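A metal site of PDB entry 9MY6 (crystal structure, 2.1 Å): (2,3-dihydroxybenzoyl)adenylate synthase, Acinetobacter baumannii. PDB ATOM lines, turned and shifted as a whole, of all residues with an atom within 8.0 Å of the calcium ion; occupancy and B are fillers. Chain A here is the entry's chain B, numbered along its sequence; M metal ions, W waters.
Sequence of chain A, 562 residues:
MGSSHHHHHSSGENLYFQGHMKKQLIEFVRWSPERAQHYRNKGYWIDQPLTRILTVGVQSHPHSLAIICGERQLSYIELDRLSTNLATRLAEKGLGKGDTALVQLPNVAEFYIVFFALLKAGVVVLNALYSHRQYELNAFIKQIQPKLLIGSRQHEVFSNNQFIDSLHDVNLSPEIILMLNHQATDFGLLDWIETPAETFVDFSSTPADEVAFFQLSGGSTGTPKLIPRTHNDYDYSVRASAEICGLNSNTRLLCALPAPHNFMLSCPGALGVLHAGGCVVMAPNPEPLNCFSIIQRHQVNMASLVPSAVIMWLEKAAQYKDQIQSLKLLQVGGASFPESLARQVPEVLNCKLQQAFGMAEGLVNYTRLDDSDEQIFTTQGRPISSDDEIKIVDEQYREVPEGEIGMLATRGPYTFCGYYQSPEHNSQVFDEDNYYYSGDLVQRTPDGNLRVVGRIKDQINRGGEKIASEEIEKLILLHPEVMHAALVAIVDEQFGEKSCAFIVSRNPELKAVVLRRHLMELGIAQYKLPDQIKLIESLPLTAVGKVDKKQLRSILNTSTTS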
ATOM      1  N   VAL A 300     -28.923  10.534 -17.411  1.00  0.00           N
ATOM      2  CA  VAL A 300     -28.446  11.855 -17.769  1.00  0.00           C
ATOM      3  C   VAL A 300     -27.160  11.734 -18.564  1.00  0.00           C
ATOM      4  O   VAL A 300     -26.242  11.000 -18.182  1.00  0.00           O
ATOM      5  CB  VAL A 300     -28.254  12.692 -16.503  1.00  0.00           C
ATOM      6  CG1 VAL A 300     -27.584  14.024 -16.855  1.00  0.00           C
ATOM      7  CG2 VAL A 300     -29.602  12.890 -15.848  1.00  0.00           C
ATOM      8  N   ASN A 301     -27.056  12.460 -19.664  1.00  0.00           N
ATOM      9  CA  ASN A 301     -25.830  12.420 -20.434  1.00  0.00           C
ATOM     10  C   ASN A 301     -25.195  13.783 -20.555  1.00  0.00           C
ATOM     11  O   ASN A 301     -24.140  13.896 -21.184  1.00  0.00           O
ATOM     12  CB  ASN A 301     -26.061  11.771 -21.823  1.00  0.00           C
ATOM     13  CG  ASN A 301     -27.231  12.415 -22.582  1.00  0.00           C
ATOM     14  OD1 ASN A 301     -27.448  13.622 -22.479  1.00  0.00           O
ATOM     15  ND2 ASN A 301     -27.946  11.623 -23.346  1.00  0.00           N
ATOM     16  N   LYS A 321     -18.389   5.707  -9.736  1.00  0.00           N
ATOM     17  CA  LYS A 321     -18.143   5.743 -11.165  1.00  0.00           C
ATOM     18  C   LYS A 321     -19.331   5.188 -11.922  1.00  0.00           C
ATOM     19  O   LYS A 321     -19.733   5.744 -12.956  1.00  0.00           O
ATOM     20  CB  LYS A 321     -16.862   4.973 -11.508  1.00  0.00           C
ATOM     21  CG  LYS A 321     -15.651   5.885 -11.738  1.00  0.00           C
ATOM     22  CD  LYS A 321     -14.428   5.131 -12.241  1.00  0.00           C
ATOM     23  N   ILE A 324     -22.448   7.463 -12.657  1.00  0.00           N
ATOM     24  CA  ILE A 324     -22.297   8.615 -13.519  1.00  0.00           C
ATOM     25  C   ILE A 324     -21.654   8.249 -14.853  1.00  0.00           C
ATOM     26  O   ILE A 324     -21.257   9.152 -15.605  1.00  0.00           O
ATOM     27  CB  ILE A 324     -21.523   9.725 -12.810  1.00  0.00           C
ATOM     28  CG1 ILE A 324     -20.122   9.232 -12.463  1.00  0.00           C
ATOM     29  CG2 ILE A 324     -22.242  10.134 -11.543  1.00  0.00           C
ATOM     30  CD1 ILE A 324     -19.126  10.363 -12.386  1.00  0.00           C
ATOM     31  N   GLN A 325     -21.535   6.959 -15.169  1.00  0.00           N
ATOM     32  CA  GLN A 325     -20.948   6.578 -16.454  1.00  0.00           C
ATOM     33  C   GLN A 325     -21.642   7.262 -17.642  1.00  0.00           C
ATOM     34  O   GLN A 325     -20.976   7.657 -18.611  1.00  0.00           O
ATOM     35  CB  GLN A 325     -21.018   5.070 -16.641  1.00  0.00           C
ATOM     36  CG  GLN A 325     -20.018   4.192 -15.811  1.00  0.00           C
ATOM     37  CD  GLN A 325     -18.494   4.490 -15.936  1.00  0.00           C
ATOM     38  OE1 GLN A 325     -18.062   5.578 -16.362  1.00  0.00           O
ATOM     39  NE2 GLN A 325     -17.681   3.497 -15.544  1.00  0.00           N
ATOM     40  N   SER A 326     -22.977   7.432 -17.582  1.00  0.00           N
ATOM     41  CA  SER A 326     -23.727   7.907 -18.756  1.00  0.00           C
ATOM     42  C   SER A 326     -23.478   9.374 -19.052  1.00  0.00           C
ATOM     43  O   SER A 326     -23.879   9.838 -20.133  1.00  0.00           O
ATOM     44  CB  SER A 326     -25.229   7.694 -18.581  1.00  0.00           C
ATOM     45  OG  SER A 326     -25.765   8.596 -17.632  1.00  0.00           O
ATOM     46  N   LEU A 327     -22.877  10.130 -18.133  1.00  0.00           N
ATOM     47  CA  LEU A 327     -22.552  11.511 -18.458  1.00  0.00           C
ATOM     48  C   LEU A 327     -21.658  11.539 -19.672  1.00  0.00           C
ATOM     49  O   LEU A 327     -20.637  10.880 -19.685  1.00  0.00           O
ATOM     50  CB  LEU A 327     -21.830  12.196 -17.320  1.00  0.00           C
ATOM     51  CG  LEU A 327     -22.655  12.775 -16.194  1.00  0.00           C
ATOM     52  CD1 LEU A 327     -21.708  13.329 -15.105  1.00  0.00           C
ATOM     53  CD2 LEU A 327     -23.496  13.835 -16.750  1.00  0.00           C
ATOM     54  N   LYS A 328     -22.031  12.311 -20.689  1.00  0.00           N
ATOM     55  CA  LYS A 328     -21.177  12.409 -21.858  1.00  0.00           C
ATOM     56  C   LYS A 328     -20.469  13.751 -21.958  1.00  0.00           C
ATOM     57  O   LYS A 328     -19.388  13.825 -22.527  1.00  0.00           O
ATOM     58  CB  LYS A 328     -22.003  12.159 -23.145  1.00  0.00           C
ATOM     59  CG  LYS A 328     -22.593  10.750 -23.166  1.00  0.00           C
ATOM     60  CD  LYS A 328     -22.691  10.199 -24.582  1.00  0.00           C
ATOM     61  CE  LYS A 328     -23.883  10.709 -25.294  1.00  0.00           C
ATOM     62  NZ  LYS A 328     -24.467   9.650 -26.199  1.00  0.00           N
ATOM     63  N   LEU A 329     -21.025  14.786 -21.373  1.00  0.00           N
ATOM     64  CA  LEU A 329     -20.501  16.126 -21.588  1.00  0.00           C
ATOM     65  C   LEU A 329     -20.820  16.921 -20.355  1.00  0.00           C
ATOM     66  O   LEU A 329     -21.947  16.859 -19.869  1.00  0.00           O
ATOM     67  CB  LEU A 329     -21.114  16.788 -22.853  1.00  0.00           C
ATOM     68  CG  LEU A 329     -20.813  18.272 -23.135  1.00  0.00           C
ATOM     69  CD1 LEU A 329     -19.329  18.459 -23.484  1.00  0.00           C
ATOM     70  CD2 LEU A 329     -21.672  18.807 -24.275  1.00  0.00           C
ATOM     71  N   PRO A 346     -12.331  14.647 -17.548  1.00  0.00           N
ATOM     72  CA  PRO A 346     -12.366  13.362 -18.261  1.00  0.00           C
ATOM     73  C   PRO A 346     -11.777  12.194 -17.475  1.00  0.00           C
ATOM     74  O   PRO A 346     -12.246  11.058 -17.619  1.00  0.00           O
ATOM     75  CB  PRO A 346     -11.554  13.647 -19.537  1.00  0.00           C
ATOM     76  CG  PRO A 346     -10.738  14.885 -19.211  1.00  0.00           C
ATOM     77  CD  PRO A 346     -11.548  15.674 -18.252  1.00  0.00           C
ATOM     78  N   LEU A 349     -14.567  12.092 -13.914  1.00  0.00           N
ATOM     79  CA  LEU A 349     -15.987  12.067 -14.254  1.00  0.00           C
ATOM     80  C   LEU A 349     -16.274  11.281 -15.520  1.00  0.00           C
ATOM     81  O   LEU A 349     -17.431  11.017 -15.822  1.00  0.00           O
ATOM     82  CB  LEU A 349     -16.532  13.494 -14.404  1.00  0.00           C
ATOM     83  CG  LEU A 349     -16.385  14.306 -13.105  1.00  0.00           C
ATOM     84  CD1 LEU A 349     -16.884  15.743 -13.236  1.00  0.00           C
ATOM     85  CD2 LEU A 349     -17.076  13.584 -11.925  1.00  0.00           C
ATOM     86  N   ASN A 350     -15.239  10.906 -16.263  1.00  0.00           N
ATOM     87  CA  ASN A 350     -15.422  10.029 -17.407  1.00  0.00           C
ATOM     88  C   ASN A 350     -16.394  10.664 -18.400  1.00  0.00           C
ATOM     89  O   ASN A 350     -17.362  10.043 -18.841  1.00  0.00           O
ATOM     90  CB  ASN A 350     -15.871   8.638 -16.931  1.00  0.00           C
ATOM     91  CG  ASN A 350     -14.882   8.029 -15.899  1.00  0.00           C
ATOM     92  OD1 ASN A 350     -13.738   8.449 -15.853  1.00  0.00           O
ATOM     93  ND2 ASN A 350     -15.329   7.091 -15.069  1.00  0.00           N
ATOM     94  N   CYS A 351     -16.132  11.911 -18.742  1.00  0.00           N
ATOM     95  CA  CYS A 351     -16.929  12.604 -19.746  1.00  0.00           C
ATOM     96  C   CYS A 351     -16.100  13.722 -20.333  1.00  0.00           C
ATOM     97  O   CYS A 351     -15.040  14.094 -19.805  1.00  0.00           O
ATOM     98  CB  CYS A 351     -18.228  13.156 -19.162  1.00  0.00           C
ATOM     99  SG  CYS A 351     -17.869  14.419 -17.915  1.00  0.00           S
ATOM    100  N   LYS A 352     -16.596  14.270 -21.440  1.00  0.00           N
ATOM    101  CA  LYS A 352     -15.943  15.346 -22.155  1.00  0.00           C
ATOM    102  C   LYS A 352     -16.119  16.645 -21.402  1.00  0.00           C
ATOM    103  O   LYS A 352     -17.132  16.861 -20.730  1.00  0.00           O
ATOM    104  CB  LYS A 352     -16.505  15.475 -23.566  1.00  0.00           C
ATOM    105  CG  LYS A 352     -15.844  16.569 -24.384  1.00  0.00           C
ATOM    106  CD  LYS A 352     -15.432  16.042 -25.745  1.00  0.00           C
ATOM    107  CE  LYS A 352     -14.978  17.171 -26.668  1.00  0.00           C
ATOM    108  NZ  LYS A 352     -13.503  17.124 -26.868  1.00  0.00           N
HETATM  109 CA    CA M   1     -19.285   8.969 -19.383  1.00  0.00          CA
HETATM  110  O   HOH W   1     -19.279   9.456 -17.113  1.00  0.00           O
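Water W1 lies within hydrogen-bond range of O of Ile 324 (2.5 Å) and O of Leu 349 (2.7 Å).
Along chain A the residues within 4 Å of the calcium ion span positions 325 to 350.
O of Asn 350 binds the calcium ion. O of Gln 325 binds the calcium ion. Water W1 is bound to the calcium ion, 2.3 Å away. The calcium ion is bound by O of Leu 327, at 2.4 Å. The calcium ion has four donor atoms within binding distance.
The backbone carbonyl oxygen of Pro 346 sits close to the side-chain amide oxygen of Asn 350. O of Val 300 sits at hydrogen-bond distance from N of Leu 327, at 3.5 Å.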
